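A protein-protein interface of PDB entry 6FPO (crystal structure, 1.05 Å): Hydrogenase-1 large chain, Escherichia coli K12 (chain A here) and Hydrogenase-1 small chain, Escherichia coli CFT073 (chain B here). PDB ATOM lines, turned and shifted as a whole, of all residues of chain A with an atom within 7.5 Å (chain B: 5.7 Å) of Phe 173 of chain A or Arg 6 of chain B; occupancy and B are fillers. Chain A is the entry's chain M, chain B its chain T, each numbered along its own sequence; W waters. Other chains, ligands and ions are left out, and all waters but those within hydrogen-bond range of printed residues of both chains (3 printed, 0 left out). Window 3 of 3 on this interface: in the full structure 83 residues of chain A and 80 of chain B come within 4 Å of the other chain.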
ATOM      1  N   VAL A 134      13.119  13.152 -30.235  1.00  0.00           N
ATOM      2  CA  VAL A 134      12.458  14.395 -30.637  1.00  0.00           C
ATOM      3  C   VAL A 134      13.445  15.332 -31.284  1.00  0.00           C
ATOM      4  O   VAL A 134      13.117  15.976 -32.279  1.00  0.00           O
ATOM      5  CB  VAL A 134      11.780  15.022 -29.384  1.00  0.00           C
ATOM      6  CG1 VAL A 134      11.266  16.417 -29.694  1.00  0.00           C
ATOM      7  CG2 VAL A 134      10.644  14.138 -28.874  1.00  0.00           C
ATOM      8  N   LEU A 135      14.648  15.479 -30.715  1.00  0.00           N
ATOM      9  CA  LEU A 135      15.555  16.422 -31.320  1.00  0.00           C
ATOM     10  C   LEU A 135      16.038  15.961 -32.689  1.00  0.00           C
ATOM     11  O   LEU A 135      16.241  16.805 -33.591  1.00  0.00           O
ATOM     12  CB  LEU A 135      16.745  16.728 -30.422  1.00  0.00           C
ATOM     13  CG  LEU A 135      16.398  17.463 -29.132  1.00  0.00           C
ATOM     14  CD1 LEU A 135      17.751  17.834 -28.462  1.00  0.00           C
ATOM     15  CD2 LEU A 135      15.446  18.661 -29.264  1.00  0.00           C
ATOM     16  N   GLN A 167       7.896  20.570 -37.960  1.00  0.00           N
ATOM     17  CA  GLN A 167       9.306  20.688 -37.705  1.00  0.00           C
ATOM     18  C   GLN A 167       9.702  22.117 -37.353  1.00  0.00           C
ATOM     19  O   GLN A 167      10.540  22.354 -36.455  1.00  0.00           O
ATOM     20  CB  GLN A 167      10.061  20.207 -38.944  1.00  0.00           C
ATOM     21  CG  GLN A 167      11.535  20.089 -38.725  1.00  0.00           C
ATOM     22  CD  GLN A 167      12.226  19.659 -40.000  1.00  0.00           C
ATOM     23  OE1 GLN A 167      12.165  20.401 -41.004  1.00  0.00           O
ATOM     24  NE2 GLN A 167      12.867  18.484 -40.021  1.00  0.00           N
ATOM     25  N   ASN A 168       9.133  23.087 -38.087  1.00  0.00           N
ATOM     26  CA  ASN A 168       9.443  24.506 -37.771  1.00  0.00           C
ATOM     27  C   ASN A 168       8.918  24.940 -36.404  1.00  0.00           C
ATOM     28  O   ASN A 168       9.573  25.772 -35.705  1.00  0.00           O
ATOM     29  CB  ASN A 168       8.847  25.401 -38.864  1.00  0.00           C
ATOM     30  CG  ASN A 168       9.651  25.330 -40.097  1.00  0.00           C
ATOM     31  OD1 ASN A 168      10.871  25.130 -40.027  1.00  0.00           O
ATOM     32  ND2 ASN A 168       9.031  25.593 -41.232  1.00  0.00           N
ATOM     33  N   ARG A 169       7.787  24.403 -35.970  1.00  0.00           N
ATOM     34  CA  ARG A 169       7.275  24.711 -34.621  1.00  0.00           C
ATOM     35  C   ARG A 169       8.299  24.213 -33.591  1.00  0.00           C
ATOM     36  O   ARG A 169       8.571  24.891 -32.585  1.00  0.00           O
ATOM     37  CB  ARG A 169       5.936  24.044 -34.454  1.00  0.00           C
ATOM     38  CG  ARG A 169       5.219  24.365 -33.198  1.00  0.00           C
ATOM     39  CD  ARG A 169       3.938  25.066 -33.478  1.00  0.00           C
ATOM     40  NE  ARG A 169       3.433  25.681 -32.257  1.00  0.00           N
ATOM     41  CZ  ARG A 169       2.220  25.478 -31.772  1.00  0.00           C
ATOM     42  NH1 ARG A 169       1.363  24.589 -32.342  1.00  0.00           N
ATOM     43  NH2 ARG A 169       1.850  26.139 -30.669  1.00  0.00           N
ATOM     44  N   LEU A 170       8.818  23.019 -33.826  1.00  0.00           N
ATOM     45  CA  LEU A 170       9.795  22.423 -32.894  1.00  0.00           C
ATOM     46  C   LEU A 170      11.079  23.231 -32.895  1.00  0.00           C
ATOM     47  O   LEU A 170      11.694  23.519 -31.851  1.00  0.00           O
ATOM     48  CB  LEU A 170      10.060  20.968 -33.239  1.00  0.00           C
ATOM     49  CG  LEU A 170      11.048  20.229 -32.347  1.00  0.00           C
ATOM     50  CD1 LEU A 170      10.605  20.223 -30.877  1.00  0.00           C
ATOM     51  CD2 LEU A 170      11.248  18.845 -32.828  1.00  0.00           C
ATOM     52  N   LYS A 171      11.514  23.626 -34.083  1.00  0.00           N
ATOM     53  CA  LYS A 171      12.722  24.435 -34.264  1.00  0.00           C
ATOM     54  C   LYS A 171      12.573  25.717 -33.468  1.00  0.00           C
ATOM     55  O   LYS A 171      13.487  26.120 -32.744  1.00  0.00           O
ATOM     56  CB  LYS A 171      12.902  24.792 -35.744  1.00  0.00           C
ATOM     57  CG  LYS A 171      13.964  24.012 -36.498  1.00  0.00           C
ATOM     58  CD  LYS A 171      15.307  24.734 -36.519  1.00  0.00           C
ATOM     59  CE  LYS A 171      16.307  24.246 -37.586  1.00  0.00           C
ATOM     60  NZ  LYS A 171      17.034  22.933 -37.380  1.00  0.00           N
ATOM     61  N   LYS A 172      11.426  26.398 -33.600  1.00  0.00           N
ATOM     62  CA  LYS A 172      11.133  27.643 -32.803  1.00  0.00           C
ATOM     63  C   LYS A 172      11.087  27.427 -31.322  1.00  0.00           C
ATOM     64  O   LYS A 172      11.580  28.249 -30.515  1.00  0.00           O
ATOM     65  CB  LYS A 172       9.769  28.280 -33.262  1.00  0.00           C
ATOM     66  CG  LYS A 172       9.300  29.553 -32.562  1.00  0.00           C
ATOM     67  CD  LYS A 172       7.922  29.963 -33.126  1.00  0.00           C
ATOM     68  CE  LYS A 172       7.778  31.414 -33.505  1.00  0.00           C
ATOM     69  NZ  LYS A 172       7.018  32.153 -32.458  1.00  0.00           N
ATOM     70  N   PHE A 173      10.504  26.340 -30.927  1.00  0.00           N
ATOM     71  CA  PHE A 173      10.380  25.996 -29.517  1.00  0.00           C
ATOM     72  C   PHE A 173      11.650  25.898 -28.794  1.00  0.00           C
ATOM     73  O   PHE A 173      11.721  26.383 -27.573  1.00  0.00           O
ATOM     74  CB  PHE A 173       9.620  24.685 -29.379  1.00  0.00           C
ATOM     75  CG  PHE A 173       9.421  24.248 -27.949  1.00  0.00           C
ATOM     76  CD1 PHE A 173       8.452  24.841 -27.149  1.00  0.00           C
ATOM     77  CD2 PHE A 173      10.190  23.245 -27.426  1.00  0.00           C
ATOM     78  CE1 PHE A 173       8.239  24.417 -25.888  1.00  0.00           C
ATOM     79  CE2 PHE A 173       9.964  22.830 -26.139  1.00  0.00           C
ATOM     80  CZ  PHE A 173       8.984  23.414 -25.385  1.00  0.00           C
ATOM     81  N   VAL A 174      12.621  25.348 -29.462  1.00  0.00           N
ATOM     82  CA  VAL A 174      13.895  25.171 -28.819  1.00  0.00           C
ATOM     83  C   VAL A 174      14.894  26.285 -29.124  1.00  0.00           C
ATOM     84  O   VAL A 174      15.955  26.256 -28.538  1.00  0.00           O
ATOM     85  CB  VAL A 174      14.526  23.798 -29.127  1.00  0.00           C
ATOM     86  CG1 VAL A 174      13.641  22.593 -28.791  1.00  0.00           C
ATOM     87  CG2 VAL A 174      14.990  23.626 -30.517  1.00  0.00           C
ATOM     88  N   GLU A 175      14.513  27.262 -29.951  1.00  0.00           N
ATOM     89  CA  GLU A 175      15.387  28.369 -30.367  1.00  0.00           C
ATOM     90  C   GLU A 175      15.759  29.287 -29.294  1.00  0.00           C
ATOM     91  O   GLU A 175      16.809  29.833 -29.395  1.00  0.00           O
ATOM     92  CB  GLU A 175      14.780  29.141 -31.575  1.00  0.00           C
ATOM     93  CG  GLU A 175      13.893  30.362 -31.317  1.00  0.00           C
ATOM     94  CD  GLU A 175      13.526  31.063 -32.614  1.00  0.00           C
ATOM     95  OE1 GLU A 175      14.030  30.703 -33.700  1.00  0.00           O
ATOM     96  OE2 GLU A 175      12.702  31.967 -32.528  1.00  0.00           O
ATOM     97  N   GLY A 176      14.896  29.520 -28.299  1.00  0.00           N
ATOM     98  CA  GLY A 176      15.295  30.390 -27.174  1.00  0.00           C
ATOM     99  C   GLY A 176      16.005  29.697 -26.020  1.00  0.00           C
ATOM    100  O   GLY A 176      16.253  30.263 -24.967  1.00  0.00           O
ATOM    101  N   GLY A 177      16.303  28.409 -26.208  1.00  0.00           N
ATOM    102  CA  GLY A 177      16.966  27.649 -25.216  1.00  0.00           C
ATOM    103  C   GLY A 177      16.063  27.184 -24.111  1.00  0.00           C
ATOM    104  O   GLY A 177      16.566  26.736 -23.163  1.00  0.00           O
ATOM    105  N   GLN A 178      14.731  27.297 -24.248  1.00  0.00           N
ATOM    106  CA  GLN A 178      13.788  26.826 -23.200  1.00  0.00           C
ATOM    107  C   GLN A 178      13.189  25.492 -23.704  1.00  0.00           C
ATOM    108  O   GLN A 178      12.117  25.428 -24.300  1.00  0.00           O
ATOM    109  CB  GLN A 178      12.678  27.817 -22.957  1.00  0.00           C
ATOM    110  CG  GLN A 178      13.164  29.138 -22.408  1.00  0.00           C
ATOM    111  CD  GLN A 178      12.007  30.071 -22.116  1.00  0.00           C
ATOM    112  OE1 GLN A 178      11.432  30.637 -23.024  1.00  0.00           O
ATOM    113  NE2 GLN A 178      11.670  30.227 -20.857  1.00  0.00           N
ATOM    114  N   LEU A 179      13.930  24.410 -23.473  1.00  0.00           N
ATOM    115  CA  LEU A 179      13.548  23.097 -24.036  1.00  0.00           C
ATOM    116  C   LEU A 179      12.413  22.411 -23.294  1.00  0.00           C
ATOM    117  O   LEU A 179      11.865  21.434 -23.786  1.00  0.00           O
ATOM    118  CB  LEU A 179      14.747  22.163 -24.160  1.00  0.00           C
ATOM    119  CG  LEU A 179      15.549  22.266 -25.444  1.00  0.00           C
ATOM    120  CD1 LEU A 179      16.178  23.652 -25.659  1.00  0.00           C
ATOM    121  CD2 LEU A 179      16.595  21.175 -25.519  1.00  0.00           C
ATOM    122  N   GLY A 180      12.028  22.938 -22.143  1.00  0.00           N
ATOM    123  CA  GLY A 180      10.861  22.439 -21.470  1.00  0.00           C
ATOM    124  C   GLY A 180      10.938  20.950 -21.162  1.00  0.00           C
ATOM    125  O   GLY A 180      11.959  20.481 -20.629  1.00  0.00           O
ATOM    126  N   ILE A 181       9.912  20.221 -21.527  1.00  0.00           N
ATOM    127  CA  ILE A 181       9.863  18.801 -21.278  1.00  0.00           C
ATOM    128  C   ILE A 181      10.954  18.041 -22.014  1.00  0.00           C
ATOM    129  O   ILE A 181      11.213  16.877 -21.672  1.00  0.00           O
ATOM    130  CB  ILE A 181       8.480  18.219 -21.598  1.00  0.00           C
ATOM    131  CG1 ILE A 181       8.002  18.497 -23.019  1.00  0.00           C
ATOM    132  CG2 ILE A 181       7.475  18.647 -20.555  1.00  0.00           C
ATOM    133  CD1 ILE A 181       6.859  17.631 -23.487  1.00  0.00           C
ATOM    134  N   PHE A 182      11.613  18.653 -22.999  1.00  0.00           N
ATOM    135  CA  PHE A 182      12.722  17.973 -23.702  1.00  0.00           C
ATOM    136  C   PHE A 182      14.103  18.214 -23.074  1.00  0.00           C
ATOM    137  O   PHE A 182      15.069  17.622 -23.515  1.00  0.00           O
ATOM    138  CB  PHE A 182      12.752  18.380 -25.174  1.00  0.00           C
ATOM    139  CG  PHE A 182      11.410  18.308 -25.854  1.00  0.00           C
ATOM    140  CD1 PHE A 182      10.593  17.182 -25.777  1.00  0.00           C
ATOM    141  CD2 PHE A 182      10.946  19.365 -26.562  1.00  0.00           C
ATOM    142  CE1 PHE A 182       9.330  17.134 -26.350  1.00  0.00           C
ATOM    143  CE2 PHE A 182       9.712  19.361 -27.148  1.00  0.00           C
ATOM    144  CZ  PHE A 182       8.909  18.258 -27.041  1.00  0.00           C
ATOM    145  N   ARG A 183      14.179  19.085 -22.065  1.00  0.00           N
ATOM    146  CA  ARG A 183      15.469  19.462 -21.531  1.00  0.00           C
ATOM    147  C   ARG A 183      16.144  18.255 -20.880  1.00  0.00           C
ATOM    148  O   ARG A 183      15.586  17.583 -20.053  1.00  0.00           O
ATOM    149  CB  ARG A 183      15.295  20.596 -20.527  1.00  0.00           C
ATOM    150  CG  ARG A 183      16.617  21.136 -19.997  1.00  0.00           C
ATOM    151  CD  ARG A 183      16.441  22.214 -18.987  1.00  0.00           C
ATOM    152  NE  ARG A 183      17.694  22.606 -18.340  1.00  0.00           N
ATOM    153  CZ  ARG A 183      18.319  23.757 -18.451  1.00  0.00           C
ATOM    154  NH1 ARG A 183      17.826  24.741 -19.186  1.00  0.00           N
ATOM    155  NH2 ARG A 183      19.445  23.943 -17.791  1.00  0.00           N
ATOM    156  N   PHE A 203       6.740  12.471 -33.772  1.00  0.00           N
ATOM    157  CA  PHE A 203       6.542  13.700 -33.027  1.00  0.00           C
ATOM    158  C   PHE A 203       5.261  14.428 -33.478  1.00  0.00           C
ATOM    159  O   PHE A 203       4.480  14.913 -32.659  1.00  0.00           O
ATOM    160  CB  PHE A 203       7.744  14.615 -33.128  1.00  0.00           C
ATOM    161  CG  PHE A 203       7.564  15.877 -32.370  1.00  0.00           C
ATOM    162  CD1 PHE A 203       7.473  15.858 -31.014  1.00  0.00           C
ATOM    163  CD2 PHE A 203       7.414  17.094 -33.023  1.00  0.00           C
ATOM    164  CE1 PHE A 203       7.250  17.040 -30.295  1.00  0.00           C
ATOM    165  CE2 PHE A 203       7.176  18.259 -32.300  1.00  0.00           C
ATOM    166  CZ  PHE A 203       7.143  18.219 -30.933  1.00  0.00           C
ATOM    167  N   LYS B   4       9.835  35.815 -28.101  1.00  0.00           N
ATOM    168  CA  LYS B   4      10.201  36.302 -26.730  1.00  0.00           C
ATOM    169  C   LYS B   4      10.232  35.079 -25.803  1.00  0.00           C
ATOM    170  O   LYS B   4       9.477  34.124 -25.999  1.00  0.00           O
ATOM    171  CB  LYS B   4       9.208  37.334 -26.164  1.00  0.00           C
ATOM    172  N   PRO B   5      11.049  35.140 -24.750  1.00  0.00           N
ATOM    173  CA  PRO B   5      11.044  34.025 -23.811  1.00  0.00           C
ATOM    174  C   PRO B   5       9.672  33.899 -23.161  1.00  0.00           C
ATOM    175  O   PRO B   5       8.919  34.861 -23.080  1.00  0.00           O
ATOM    176  CB  PRO B   5      12.117  34.407 -22.805  1.00  0.00           C
ATOM    177  CG  PRO B   5      13.030  35.315 -23.562  1.00  0.00           C
ATOM    178  CD  PRO B   5      12.129  36.102 -24.472  1.00  0.00           C
ATOM    179  N   ARG B   6       9.342  32.692 -22.760  1.00  0.00           N
ATOM    180  CA  ARG B   6       8.076  32.399 -22.085  1.00  0.00           C
ATOM    181  C   ARG B   6       8.334  32.268 -20.590  1.00  0.00           C
ATOM    182  O   ARG B   6       9.421  31.911 -20.142  1.00  0.00           O
ATOM    183  CB  ARG B   6       7.485  31.109 -22.730  1.00  0.00           C
ATOM    184  CG  ARG B   6       6.950  31.326 -24.142  1.00  0.00           C
ATOM    185  CD  ARG B   6       6.730  30.032 -24.980  1.00  0.00           C
ATOM    186  NE  ARG B   6       8.030  29.441 -25.474  1.00  0.00           N
ATOM    187  CZ  ARG B   6       8.574  28.275 -25.105  1.00  0.00           C
ATOM    188  NH1 ARG B   6       8.018  27.535 -24.185  1.00  0.00           N
ATOM    189  NH2 ARG B   6       9.720  27.885 -25.642  1.00  0.00           N
ATOM    190  N   ILE B   7       7.283  32.471 -19.820  1.00  0.00           N
ATOM    191  CA  ILE B   7       7.405  32.471 -18.374  1.00  0.00           C
ATOM    192  C   ILE B   7       7.740  31.068 -17.864  1.00  0.00           C
ATOM    193  O   ILE B   7       7.039  30.109 -18.189  1.00  0.00           O
ATOM    194  CB  ILE B   7       6.149  33.006 -17.670  1.00  0.00           C
ATOM    195  CG1 ILE B   7       6.337  33.041 -16.133  1.00  0.00           C
ATOM    196  CG2 ILE B   7       4.894  32.176 -17.950  1.00  0.00           C
ATOM    197  CD1 ILE B   7       5.925  34.247 -15.369  1.00  0.00           C
ATOM    198  N   PRO B   8       8.762  30.920 -17.020  1.00  0.00           N
ATOM    199  CA  PRO B   8       9.106  29.593 -16.488  1.00  0.00           C
ATOM    200  C   PRO B   8       8.073  29.110 -15.506  1.00  0.00           C
ATOM    201  O   PRO B   8       7.621  29.845 -14.627  1.00  0.00           O
ATOM    202  CB  PRO B   8      10.453  29.814 -15.826  1.00  0.00           C
ATOM    203  CG  PRO B   8      10.852  31.116 -16.179  1.00  0.00           C
ATOM    204  CD  PRO B   8       9.767  31.924 -16.678  1.00  0.00           C
ATOM    205  N   ILE B  36       1.732  24.763 -23.768  1.00  0.00           N
ATOM    206  CA  ILE B  36       3.092  24.292 -23.561  1.00  0.00           C
ATOM    207  C   ILE B  36       4.032  24.873 -24.637  1.00  0.00           C
ATOM    208  O   ILE B  36       5.187  25.259 -24.314  1.00  0.00           O
ATOM    209  CB  ILE B  36       3.106  22.718 -23.533  1.00  0.00           C
ATOM    210  CG1 ILE B  36       2.360  22.248 -22.312  1.00  0.00           C
ATOM    211  CG2 ILE B  36       4.514  22.181 -23.618  1.00  0.00           C
ATOM    212  CD1 ILE B  36       2.043  20.760 -22.339  1.00  0.00           C
ATOM    213  N   LEU B  37       3.603  24.905 -25.882  1.00  0.00           N
ATOM    214  CA  LEU B  37       4.533  25.321 -26.951  1.00  0.00           C
ATOM    215  C   LEU B  37       4.696  26.812 -27.000  1.00  0.00           C
ATOM    216  O   LEU B  37       5.796  27.311 -27.281  1.00  0.00           O
ATOM    217  CB  LEU B  37       4.067  24.762 -28.305  1.00  0.00           C
ATOM    218  CG  LEU B  37       4.265  23.212 -28.479  1.00  0.00           C
ATOM    219  CD1 LEU B  37       3.720  22.775 -29.789  1.00  0.00           C
ATOM    220  CD2 LEU B  37       5.698  22.723 -28.336  1.00  0.00           C
ATOM    221  N   SER B  38       3.620  27.564 -26.703  1.00  0.00           N
ATOM    222  CA  SER B  38       3.545  28.975 -27.029  1.00  0.00           C
ATOM    223  C   SER B  38       3.269  29.932 -25.893  1.00  0.00           C
ATOM    224  O   SER B  38       3.639  31.134 -25.983  1.00  0.00           O
ATOM    225  CB  SER B  38       2.545  29.208 -28.203  1.00  0.00           C
ATOM    226  OG  SER B  38       2.965  28.502 -29.378  1.00  0.00           O
ATOM    227  N   LEU B  39       2.647  29.499 -24.817  1.00  0.00           N
ATOM    228  CA  LEU B  39       2.173  30.405 -23.801  1.00  0.00           C
ATOM    229  C   LEU B  39       3.093  30.483 -22.570  1.00  0.00           C
ATOM    230  O   LEU B  39       3.276  31.559 -21.982  1.00  0.00           O
ATOM    231  CB  LEU B  39       0.768  29.978 -23.362  1.00  0.00           C
ATOM    232  CG  LEU B  39      -0.025  30.992 -22.573  1.00  0.00           C
ATOM    233  CD1 LEU B  39      -0.362  32.277 -23.347  1.00  0.00           C
ATOM    234  CD2 LEU B  39      -1.301  30.325 -22.081  1.00  0.00           C
ATOM    235  N   ILE B  40       3.593  29.352 -22.133  1.00  0.00           N
ATOM    236  CA  ILE B  40       4.448  29.230 -20.967  1.00  0.00           C
ATOM    237  C   ILE B  40       5.640  28.382 -21.350  1.00  0.00           C
ATOM    238  O   ILE B  40       5.701  27.820 -22.414  1.00  0.00           O
ATOM    239  CB  ILE B  40       3.675  28.585 -19.742  1.00  0.00           C
ATOM    240  CG1 ILE B  40       3.343  27.045 -20.016  1.00  0.00           C
ATOM    241  CG2 ILE B  40       2.457  29.411 -19.352  1.00  0.00           C
ATOM    242  CD1 ILE B  40       2.713  26.270 -18.904  1.00  0.00           C
ATOM    243  N   SER B  41       6.624  28.331 -20.419  1.00  0.00           N
ATOM    244  CA  SER B  41       7.697  27.364 -20.537  1.00  0.00           C
ATOM    245  C   SER B  41       7.544  26.364 -19.385  1.00  0.00           C
ATOM    246  O   SER B  41       7.857  26.664 -18.239  1.00  0.00           O
ATOM    247  CB  SER B  41       9.080  28.051 -20.494  1.00  0.00           C
ATOM    248  OG  SER B  41      10.104  27.113 -20.847  1.00  0.00           O
ATOM    249  N   LEU B  42       6.989  25.191 -19.720  1.00  0.00           N
ATOM    250  CA  LEU B  42       6.758  24.167 -18.708  1.00  0.00           C
ATOM    251  C   LEU B  42       8.068  23.421 -18.516  1.00  0.00           C
ATOM    252  O   LEU B  42       8.456  22.554 -19.293  1.00  0.00           O
ATOM    253  CB  LEU B  42       5.618  23.222 -19.146  1.00  0.00           C
ATOM    254  CG  LEU B  42       5.286  22.132 -18.119  1.00  0.00           C
ATOM    255  CD1 LEU B  42       4.897  22.649 -16.759  1.00  0.00           C
ATOM    256  CD2 LEU B  42       4.226  21.216 -18.655  1.00  0.00           C
HETATM  257  O   HOH W   1       9.585  25.557 -22.970  1.00  0.00           O
HETATM  258  O   HOH W   2       7.591  21.863 -21.823  1.00  0.00           O
HETATM  259  O   HOH W   3      10.174  29.399 -28.229  1.00  0.00           O
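Of the printed residues of chain B, Arg 169 of chain A touches Leu 37 (3.5 Å) and Ser 38 (2.9 Å).
Phe 173 of chain A touches just these residues of chain B: Arg 6, Ile 36 and Leu 37.
Of the printed residues of chain B, Gly 180 of chain A touches Leu 42.
Of the printed residues of chain B, Ile 181 of chain A touches Leu 42 (3.5 Å).
Of the printed residues of chain A, Ser 41 of chain B touches Gln 178.
The nearest residue of chain B that does not touch Phe 173 of chain A is Ile 40 of chain B (5.5 Å).
The nearest residue of chain A that does not touch Arg 6 of chain B is Lys 172 of chain A (5.2 Å).
The nearest printed residue of chain B that does not touch Arg 169 of chain A is Ile 36 of chain B (6.5 Å).
Of the 20 printed residues of chain A, 5 touch a printed residue of chain B.
Printed residues of chain A that touch a printed residue of chain B: Arg 169, Phe 173, Gln 178, Gly 180 and Ile 181.
Hydrophobic or aromatic side chains of chain A that line the printed part of chain B: Phe 173.
Hydrophobic or aromatic side chains of chain B within 4 Å of the printed part of chain A: Pro 5 and Leu 37.
Among the printed residues, no Asp or Glu carboxylate lies within 4 Å of a Lys or Arg side-chain nitrogen of the other chain.
Among the printed residues, merely in contact across the chains: Arg 169 of chain A with Leu 37 of chain B, Phe 173 of chain A with Ile 36 of chain B, Phe 173 of chain A with Leu 37 of chain B, Gln 178 of chain A with Pro 5 of chain B, Gly 180 of chain A with Leu 42 of chain B and Ile 181 of chain A with Leu 42 of chain B.
The backbone carbonyl oxygen (O) of Ile 40 of chain B lies within hydrogen-bond range of the guanidinium group (NH1) of Arg 6 of chain B, 2.9 Å away.
O of Ile 7 of chain B lies within hydrogen-bond range of N of Ser 41 of chain B (2.9 Å).
Water W1 lies within hydrogen-bond range of the side-chain hydroxyl (OG) of Ser 41 of chain B, the guanidinium group (NH1) of Arg 6 of chain B and the backbone carbonyl oxygen (O) of Gln 178 of chain A.
Water W2 bridges the backbone carbonyl oxygen (O) of Leu 42 of chain B (2.8 Å) and the backbone NH (N) of Ile 181 of chain A (2.9 Å).
Water W3 lies within hydrogen-bond range of O of Lys 172 of chain A (2.9 Å), NH2 of Arg 6 of chain B (3.0 Å) and O of Phe 173 of chain A (3.5 Å).
The backbone carbonyl oxygen of Phe 173 of chain A sits at hydrogen-bond distance from the guanidinium group of Arg 6 of chain B (3.2 Å).
NE2 of Gln 178 of chain A lies within hydrogen-bond range of O of Arg 6 of chain B (2.9 Å).
The guanidinium group (NH2) of Arg 169 of chain A lies within hydrogen-bond range of the side-chain hydroxyl (OG) of Ser 38 of chain B.
NE2 of Gln 178 of chain A lies close to OG of Ser 41 of chain B (3.5 Å).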
